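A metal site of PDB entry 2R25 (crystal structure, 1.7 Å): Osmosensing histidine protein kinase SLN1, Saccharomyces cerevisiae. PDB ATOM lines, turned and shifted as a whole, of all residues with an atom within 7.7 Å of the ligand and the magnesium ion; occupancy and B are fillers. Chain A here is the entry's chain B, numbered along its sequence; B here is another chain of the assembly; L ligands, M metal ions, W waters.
F2 of the ligand sits at hydrogen-bond distance from N of Gln 61 of chain A.
OD1 of Asp 59 is bound to BE1 of the ligand, 1.7 Å away.
N of Val 60 sits at hydrogen-bond distance from F2 of the ligand (3.2 Å).
N of Ala 89 sits at hydrogen-bond distance from F3 of the ligand, at 2.7 Å.
The side-chain hydroxyl of Thr 88 is in hydrogen-bond range of a fluorine (F2) of the ligand (2.6 Å).
NE2 of His 64 of chain B sits at hydrogen-bond distance from F2 of the ligand (2.7 Å).
The side-chain amino group of Lys 110 lies within hydrogen-bond range of a fluorine (F3) of the ligand (2.9 Å).
Water W1 bridges the side-chain carboxylate of Glu 9 (2.6 Å) and the side-chain amino group of Lys 110 (3.5 Å).
The magnesium ion is bound by a fluorine (F1) of the ligand (2.0 Å), water W2 (2.0 Å), the side-chain carboxylate (OD2) of Asp 10 (2.1 Å), the side-chain carboxylate (OD2) of Asp 59 (2.1 Å), water W1 (2.1 Å) and the backbone carbonyl oxygen (O) of Gln 61 of chain A (2.1 Å).
The magnesium ion has six donor atoms within binding distance.
Hydrophobic or aromatic side chains within 4 Å of the ligand: Val 60, Ala 89 and His 64 of chain B.
Seven residues have an atom within 4 Å of the ligand: Asp 59, Val 60, Gln 61 of chain A, Thr 88, Ala 89, Lys 110 and His 64 of chain B.
The backbone carbonyl oxygen (O) of Ala 89 is in hydrogen-bond range of the side-chain amino group (NZ) of Lys 67 of chain B, at 2.9 Å.
The side-chain carboxylate of Glu 9 is in salt-bridge range of the side-chain amino group of Lys 110 (2.6 Å).
The backbone NH (N) of Phe 90 sits close to the side-chain hydroxyl (OG1) of Thr 88 (3.2 Å).
The side-chain amide nitrogen (NE2) of Gln 61 of chain A sits at hydrogen-bond distance from the side-chain amide oxygen (OD1) of Asn 61 of chain B (3.1 Å).
OD1 of Asp 59 lies close to NZ of Lys 110 (3.7 Å).
N of Gly 67 of chain A sits at hydrogen-bond distance from O of Val 60 (2.7 Å).
N of Asp 59 lies within hydrogen-bond range of O of Val 8 (2.9 Å).
O of Thr 88 lies within hydrogen-bond range of N of Lys 110, 3.0 Å away.
Three residues have an atom within 4 Å of the magnesium ion: Asp 10, Asp 59 and Gln 61 of chain A.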
ATOM      1  N   VAL A   8      -9.518  17.162 -14.503  1.00  0.00           N
ATOM      2  CA  VAL A   8      -9.537  18.131 -13.426  1.00  0.00           C
ATOM      3  C   VAL A   8      -9.834  17.362 -12.136  1.00  0.00           C
ATOM      4  O   VAL A   8     -10.918  16.740 -11.988  1.00  0.00           O
ATOM      5  CB  VAL A   8     -10.617  19.180 -13.648  1.00  0.00           C
ATOM      6  CG1 VAL A   8     -10.497  20.306 -12.578  1.00  0.00           C
ATOM      7  CG2 VAL A   8     -10.607  19.689 -15.106  1.00  0.00           C
ATOM      8  N   GLU A   9      -8.893  17.424 -11.188  1.00  0.00           N
ATOM      9  CA  GLU A   9      -8.872  16.460 -10.085  1.00  0.00           C
ATOM     10  C   GLU A   9      -7.802  16.934  -9.086  1.00  0.00           C
ATOM     11  O   GLU A   9      -6.656  17.138  -9.484  1.00  0.00           O
ATOM     12  CB  GLU A   9      -8.512  15.078 -10.669  1.00  0.00           C
ATOM     13  CG  GLU A   9      -8.286  13.978  -9.620  1.00  0.00           C
ATOM     14  CD  GLU A   9      -9.448  13.808  -8.674  1.00  0.00           C
ATOM     15  OE1 GLU A   9      -9.292  14.066  -7.453  1.00  0.00           O
ATOM     16  OE2 GLU A   9     -10.539  13.385  -9.129  1.00  0.00           O
ATOM     17  N   ASP A  10      -8.181  17.115  -7.828  1.00  0.00           N
ATOM     18  CA  ASP A  10      -7.264  17.570  -6.761  1.00  0.00           C
ATOM     19  C   ASP A  10      -6.500  16.401  -6.121  1.00  0.00           C
ATOM     20  O   ASP A  10      -5.452  16.633  -5.523  1.00  0.00           O
ATOM     21  CB  ASP A  10      -7.948  18.444  -5.689  1.00  0.00           C
ATOM     22  CG  ASP A  10      -9.036  17.720  -4.914  1.00  0.00           C
ATOM     23  OD1 ASP A  10      -9.068  17.763  -3.667  1.00  0.00           O
ATOM     24  OD2 ASP A  10      -9.922  17.139  -5.570  1.00  0.00           O
ATOM     25  N   ASN A  11      -7.003  15.177  -6.284  1.00  0.00           N
ATOM     26  CA  ASN A  11      -6.295  14.018  -5.686  1.00  0.00           C
ATOM     27  C   ASN A  11      -5.329  13.355  -6.670  1.00  0.00           C
ATOM     28  O   ASN A  11      -5.754  12.801  -7.690  1.00  0.00           O
ATOM     29  CB  ASN A  11      -7.291  13.002  -5.164  1.00  0.00           C
ATOM     30  CG  ASN A  11      -6.606  11.857  -4.334  1.00  0.00           C
ATOM     31  OD1 ASN A  11      -5.615  11.271  -4.750  1.00  0.00           O
ATOM     32  ND2 ASN A  11      -7.143  11.569  -3.120  1.00  0.00           N
ATOM     33  N   ASN A  14      -5.889   9.688  -7.943  1.00  0.00           N
ATOM     34  CA  ASN A  14      -6.937   9.629  -8.971  1.00  0.00           C
ATOM     35  C   ASN A  14      -6.454  10.149 -10.299  1.00  0.00           C
ATOM     36  O   ASN A  14      -6.739   9.538 -11.337  1.00  0.00           O
ATOM     37  CB  ASN A  14      -8.185  10.333  -8.489  1.00  0.00           C
ATOM     38  CG  ASN A  14      -8.766   9.646  -7.301  1.00  0.00           C
ATOM     39  OD1 ASN A  14      -8.560  10.072  -6.199  1.00  0.00           O
ATOM     40  ND2 ASN A  14      -9.389   8.497  -7.518  1.00  0.00           N
ATOM     41  N   CYS A  34      -5.543  20.951 -11.035  1.00  0.00           N
ATOM     42  CA  CYS A  34      -5.755  20.550  -9.650  1.00  0.00           C
ATOM     43  C   CYS A  34      -6.967  21.153  -8.962  1.00  0.00           C
ATOM     44  O   CYS A  34      -7.340  20.733  -7.860  1.00  0.00           O
ATOM     45  CB  CYS A  34      -4.511  20.826  -8.808  1.00  0.00           C
ATOM     46  SG  CYS A  34      -3.185  19.752  -9.388  1.00  0.00           S
ATOM     47  N   MET A  58     -14.250  16.090 -14.987  1.00  0.00           N
ATOM     48  CA  MET A  58     -14.315  17.085 -13.948  1.00  0.00           C
ATOM     49  C   MET A  58     -14.709  16.517 -12.596  1.00  0.00           C
ATOM     50  O   MET A  58     -15.835  16.082 -12.377  1.00  0.00           O
ATOM     51  CB  MET A  58     -15.265  18.216 -14.373  1.00  0.00           C
ATOM     52  CG  MET A  58     -15.489  19.330 -13.367  1.00  0.00           C
ATOM     53  SD  MET A  58     -14.138  20.552 -13.493  1.00  0.00           S
ATOM     54  CE  MET A  58     -14.575  21.382 -15.076  1.00  0.00           C
ATOM     55  N   ASP A  59     -13.769  16.606 -11.660  1.00  0.00           N
ATOM     56  CA  ASP A  59     -14.044  16.271 -10.286  1.00  0.00           C
ATOM     57  C   ASP A  59     -15.011  17.352  -9.701  1.00  0.00           C
ATOM     58  O   ASP A  59     -15.011  18.526 -10.136  1.00  0.00           O
ATOM     59  CB  ASP A  59     -12.708  16.198  -9.568  1.00  0.00           C
ATOM     60  CG  ASP A  59     -12.848  15.895  -8.084  1.00  0.00           C
ATOM     61  OD1 ASP A  59     -13.751  15.105  -7.721  1.00  0.00           O
ATOM     62  OD2 ASP A  59     -12.004  16.410  -7.307  1.00  0.00           O
ATOM     63  N   VAL A  60     -15.799  16.978  -8.718  1.00  0.00           N
ATOM     64  CA  VAL A  60     -16.647  17.987  -8.046  1.00  0.00           C
ATOM     65  C   VAL A  60     -15.961  18.732  -6.899  1.00  0.00           C
ATOM     66  O   VAL A  60     -15.781  19.940  -7.017  1.00  0.00           O
ATOM     67  CB  VAL A  60     -17.943  17.414  -7.542  1.00  0.00           C
ATOM     68  CG1 VAL A  60     -18.771  18.536  -6.887  1.00  0.00           C
ATOM     69  CG2 VAL A  60     -18.643  16.800  -8.694  1.00  0.00           C
ATOM     70  N   GLN A  61     -15.600  18.077  -5.800  1.00  0.00           N
ATOM     71  CA  GLN A  61     -14.969  18.853  -4.689  1.00  0.00           C
ATOM     72  C   GLN A  61     -13.529  19.108  -4.917  1.00  0.00           C
ATOM     73  O   GLN A  61     -12.739  18.181  -5.029  1.00  0.00           O
ATOM     74  CB  GLN A  61     -15.098  18.150  -3.313  1.00  0.00           C
ATOM     75  CG  GLN A  61     -16.438  17.698  -2.889  1.00  0.00           C
ATOM     76  CD  GLN A  61     -16.578  17.563  -1.358  1.00  0.00           C
ATOM     77  OE1 GLN A  61     -17.692  17.525  -0.842  1.00  0.00           O
ATOM     78  NE2 GLN A  61     -15.457  17.499  -0.628  1.00  0.00           N
ATOM     79  N   MET A  62     -13.145  20.370  -4.895  1.00  0.00           N
ATOM     80  CA  MET A  62     -11.768  20.777  -5.094  1.00  0.00           C
ATOM     81  C   MET A  62     -11.632  22.135  -4.395  1.00  0.00           C
ATOM     82  O   MET A  62     -12.638  22.885  -4.293  1.00  0.00           O
ATOM     83  CB  MET A  62     -11.440  20.928  -6.582  1.00  0.00           C
ATOM     84  CG  MET A  62     -11.715  19.667  -7.506  1.00  0.00           C
ATOM     85  SD  MET A  62     -11.269  20.027  -9.194  1.00  0.00           S
ATOM     86  CE  MET A  62     -12.756  20.931  -9.741  1.00  0.00           C
ATOM     87  N   PRO A  63     -10.425  22.459  -3.927  1.00  0.00           N
ATOM     88  CA  PRO A  63     -10.255  23.769  -3.260  1.00  0.00           C
ATOM     89  C   PRO A  63     -10.398  24.919  -4.281  1.00  0.00           C
ATOM     90  O   PRO A  63     -10.251  24.711  -5.485  1.00  0.00           O
ATOM     91  CB  PRO A  63      -8.817  23.726  -2.716  1.00  0.00           C
ATOM     92  CG  PRO A  63      -8.285  22.286  -2.928  1.00  0.00           C
ATOM     93  CD  PRO A  63      -9.157  21.692  -4.028  1.00  0.00           C
ATOM     94  N   GLY A  67     -16.065  21.758  -9.057  1.00  0.00           N
ATOM     95  CA  GLY A  67     -16.297  21.402 -10.462  1.00  0.00           C
ATOM     96  C   GLY A  67     -17.617  21.917 -11.018  1.00  0.00           C
ATOM     97  O   GLY A  67     -17.756  22.127 -12.228  1.00  0.00           O
ATOM     98  N   LEU A  87     -16.322  13.338 -12.976  1.00  0.00           N
ATOM     99  CA  LEU A  87     -15.546  12.175 -12.527  1.00  0.00           C
ATOM    100  C   LEU A  87     -15.168  12.356 -11.075  1.00  0.00           C
ATOM    101  O   LEU A  87     -14.227  13.093 -10.725  1.00  0.00           O
ATOM    102  CB  LEU A  87     -14.345  11.944 -13.458  1.00  0.00           C
ATOM    103  CG  LEU A  87     -13.757  10.552 -13.757  1.00  0.00           C
ATOM    104  CD1 LEU A  87     -12.262  10.611 -14.147  1.00  0.00           C
ATOM    105  CD2 LEU A  87     -13.960   9.632 -12.618  1.00  0.00           C
ATOM    106  N   THR A  88     -15.919  11.707 -10.182  1.00  0.00           N
ATOM    107  CA  THR A  88     -16.041  12.193  -8.811  1.00  0.00           C
ATOM    108  C   THR A  88     -16.300  11.055  -7.815  1.00  0.00           C
ATOM    109  O   THR A  88     -16.873  10.020  -8.212  1.00  0.00           O
ATOM    110  CB  THR A  88     -17.207  13.221  -8.751  1.00  0.00           C
ATOM    111  OG1 THR A  88     -17.505  13.522  -7.365  1.00  0.00           O
ATOM    112  CG2 THR A  88     -18.466  12.584  -9.374  1.00  0.00           C
ATOM    113  N   ALA A  89     -15.926  11.224  -6.537  1.00  0.00           N
ATOM    114  CA  ALA A  89     -16.235  10.135  -5.559  1.00  0.00           C
ATOM    115  C   ALA A  89     -17.742  10.063  -5.183  1.00  0.00           C
ATOM    116  O   ALA A  89     -18.198   9.078  -4.576  1.00  0.00           O
ATOM    117  CB  ALA A  89     -15.330  10.213  -4.312  1.00  0.00           C
ATOM    118  N   PHE A  90     -18.501  11.097  -5.551  1.00  0.00           N
ATOM    119  CA  PHE A  90     -19.964  11.062  -5.466  1.00  0.00           C
ATOM    120  C   PHE A  90     -20.541   9.941  -6.353  1.00  0.00           C
ATOM    121  O   PHE A  90     -20.089   9.754  -7.484  1.00  0.00           O
ATOM    122  CB  PHE A  90     -20.504  12.438  -5.863  1.00  0.00           C
ATOM    123  CG  PHE A  90     -20.278  13.507  -4.775  1.00  0.00           C
ATOM    124  CD1 PHE A  90     -20.639  13.290  -3.423  1.00  0.00           C
ATOM    125  CD2 PHE A  90     -19.709  14.736  -5.110  1.00  0.00           C
ATOM    126  CE1 PHE A  90     -20.414  14.291  -2.444  1.00  0.00           C
ATOM    127  CE2 PHE A  90     -19.486  15.740  -4.140  1.00  0.00           C
ATOM    128  CZ  PHE A  90     -19.822  15.513  -2.805  1.00  0.00           C
ATOM    129  N   ASN A  95     -26.342  14.556  -6.451  1.00  0.00           N
ATOM    130  CA  ASN A  95     -25.089  14.943  -7.109  1.00  0.00           C
ATOM    131  C   ASN A  95     -25.125  14.814  -8.644  1.00  0.00           C
ATOM    132  O   ASN A  95     -24.644  15.693  -9.366  1.00  0.00           O
ATOM    133  CB  ASN A  95     -23.915  14.138  -6.527  1.00  0.00           C
ATOM    134  CG  ASN A  95     -23.616  14.525  -5.078  1.00  0.00           C
ATOM    135  OD1 ASN A  95     -23.801  13.721  -4.147  1.00  0.00           O
ATOM    136  ND2 ASN A  95     -23.179  15.754  -4.871  1.00  0.00           N
ATOM    137  N   LEU A 108     -19.573  10.032 -14.166  1.00  0.00           N
ATOM    138  CA  LEU A 108     -18.913   8.783 -13.752  1.00  0.00           C
ATOM    139  C   LEU A 108     -18.574   8.869 -12.264  1.00  0.00           C
ATOM    140  O   LEU A 108     -18.052   9.892 -11.788  1.00  0.00           O
ATOM    141  CB  LEU A 108     -17.600   8.569 -14.511  1.00  0.00           C
ATOM    142  CG  LEU A 108     -17.647   8.482 -16.040  1.00  0.00           C
ATOM    143  CD1 LEU A 108     -16.255   8.393 -16.542  1.00  0.00           C
ATOM    144  CD2 LEU A 108     -18.411   7.189 -16.384  1.00  0.00           C
ATOM    145  N   LYS A 110     -16.316   7.232  -9.079  1.00  0.00           N
ATOM    146  CA  LYS A 110     -15.081   6.532  -8.810  1.00  0.00           C
ATOM    147  C   LYS A 110     -15.464   5.318  -7.962  1.00  0.00           C
ATOM    148  O   LYS A 110     -16.388   5.410  -7.150  1.00  0.00           O
ATOM    149  CB  LYS A 110     -14.054   7.371  -7.999  1.00  0.00           C
ATOM    150  CG  LYS A 110     -13.482   8.642  -8.683  1.00  0.00           C
ATOM    151  CD  LYS A 110     -12.840   9.633  -7.637  1.00  0.00           C
ATOM    152  CE  LYS A 110     -12.378  10.868  -8.382  1.00  0.00           C
ATOM    153  NZ  LYS A 110     -11.920  11.921  -7.460  1.00  0.00           N
ATOM    154  N   ASN B  61     -14.604  17.795   3.446  1.00  0.00           N
ATOM    155  CA  ASN B  61     -13.669  17.798   2.292  1.00  0.00           C
ATOM    156  C   ASN B  61     -12.534  16.778   2.452  1.00  0.00           C
ATOM    157  O   ASN B  61     -12.067  16.170   1.471  1.00  0.00           O
ATOM    158  CB  ASN B  61     -13.037  19.191   2.102  1.00  0.00           C
ATOM    159  CG  ASN B  61     -14.040  20.242   1.646  1.00  0.00           C
ATOM    160  OD1 ASN B  61     -15.159  19.924   1.221  1.00  0.00           O
ATOM    161  ND2 ASN B  61     -13.641  21.483   1.712  1.00  0.00           N
ATOM    162  N   HIS B  64     -14.034  13.271   1.868  1.00  0.00           N
ATOM    163  CA  HIS B  64     -14.325  13.072   0.462  1.00  0.00           C
ATOM    164  C   HIS B  64     -13.040  12.876  -0.341  1.00  0.00           C
ATOM    165  O   HIS B  64     -12.966  12.050  -1.268  1.00  0.00           O
ATOM    166  CB  HIS B  64     -15.121  14.268  -0.069  1.00  0.00           C
ATOM    167  CG  HIS B  64     -15.646  14.073  -1.441  1.00  0.00           C
ATOM    168  ND1 HIS B  64     -16.828  13.399  -1.693  1.00  0.00           N
ATOM    169  CD2 HIS B  64     -15.186  14.481  -2.655  1.00  0.00           C
ATOM    170  CE1 HIS B  64     -17.068  13.407  -2.992  1.00  0.00           C
ATOM    171  NE2 HIS B  64     -16.105  14.079  -3.597  1.00  0.00           N
ATOM    172  N   PHE B  65     -12.003  13.635   0.014  1.00  0.00           N
ATOM    173  CA  PHE B  65     -10.711  13.490  -0.632  1.00  0.00           C
ATOM    174  C   PHE B  65     -10.132  12.061  -0.537  1.00  0.00           C
ATOM    175  O   PHE B  65      -9.802  11.436  -1.548  1.00  0.00           O
ATOM    176  CB  PHE B  65      -9.768  14.520  -0.031  1.00  0.00           C
ATOM    177  CG  PHE B  65      -8.366  14.424  -0.526  1.00  0.00           C
ATOM    178  CD1 PHE B  65      -7.993  15.070  -1.710  1.00  0.00           C
ATOM    179  CD2 PHE B  65      -7.409  13.791   0.231  1.00  0.00           C
ATOM    180  CE1 PHE B  65      -6.621  15.030  -2.170  1.00  0.00           C
ATOM    181  CE2 PHE B  65      -6.095  13.731  -0.197  1.00  0.00           C
ATOM    182  CZ  PHE B  65      -5.687  14.331  -1.379  1.00  0.00           C
ATOM    183  N   LYS B  67     -11.737   9.385   0.357  1.00  0.00           N
ATOM    184  CA  LYS B  67     -12.708   8.430  -0.236  1.00  0.00           C
ATOM    185  C   LYS B  67     -12.324   8.098  -1.707  1.00  0.00           C
ATOM    186  O   LYS B  67     -12.306   6.937  -2.146  1.00  0.00           O
ATOM    187  CB  LYS B  67     -14.135   9.001  -0.159  1.00  0.00           C
ATOM    188  CG  LYS B  67     -15.208   8.051  -0.714  1.00  0.00           C
ATOM    189  CD  LYS B  67     -16.479   8.799  -0.993  1.00  0.00           C
ATOM    190  CE  LYS B  67     -17.533   7.898  -1.640  1.00  0.00           C
ATOM    191  NZ  LYS B  67     -18.838   8.610  -1.745  1.00  0.00           N
ATOM    192  N   GLY B  68     -11.988   9.118  -2.488  1.00  0.00           N
ATOM    193  CA  GLY B  68     -11.773   8.925  -3.909  1.00  0.00           C
ATOM    194  C   GLY B  68     -10.554   8.037  -4.217  1.00  0.00           C
ATOM    195  O   GLY B  68     -10.621   7.126  -5.037  1.00  0.00           O
ATOM    196  N   SER B  69      -9.479   8.269  -3.495  1.00  0.00           N
ATOM    197  CA  SER B  69      -8.255   7.518  -3.649  1.00  0.00           C
ATOM    198  C   SER B  69      -8.352   6.104  -3.081  1.00  0.00           C
ATOM    199  O   SER B  69      -7.954   5.126  -3.775  1.00  0.00           O
ATOM    200  CB  SER B  69      -7.023   8.288  -3.147  1.00  0.00           C
ATOM    201  OG  SER B  69      -7.077   8.533  -1.751  1.00  0.00           O
ATOM    202  N   GLN B  86     -17.759  12.294   5.356  1.00  0.00           N
ATOM    203  CA  GLN B  86     -18.328  13.337   4.506  1.00  0.00           C
ATOM    204  C   GLN B  86     -19.770  13.667   4.896  1.00  0.00           C
ATOM    205  O   GLN B  86     -20.144  14.826   5.073  1.00  0.00           O
ATOM    206  CB  GLN B  86     -18.256  12.908   3.033  1.00  0.00           C
ATOM    207  CG  GLN B  86     -18.050  14.082   2.067  1.00  0.00           C
ATOM    208  CD  GLN B  86     -19.327  14.678   1.512  1.00  0.00           C
ATOM    209  OE1 GLN B  86     -19.297  15.453   0.550  1.00  0.00           O
ATOM    210  NE2 GLN B  86     -20.460  14.328   2.114  1.00  0.00           N
HETATM  211 BE1  LIG L   1     -14.302  14.624  -6.199  1.00  0.00          BE
HETATM  212  F1  LIG L   1     -13.531  15.312  -5.127  1.00  0.00           F
HETATM  213  F2  LIG L   1     -15.750  15.000  -6.156  1.00  0.00           F
HETATM  214  F3  LIG L   1     -14.130  13.152  -6.084  1.00  0.00           F
HETATM  215 MG    MG M   1     -11.772  16.287  -5.225  1.00  0.00          MG
HETATM  216  O   HOH W   1     -10.741  14.444  -5.347  1.00  0.00           O
HETATM  217  O   HOH W   2     -11.312  16.281  -3.251  1.00  0.00           O
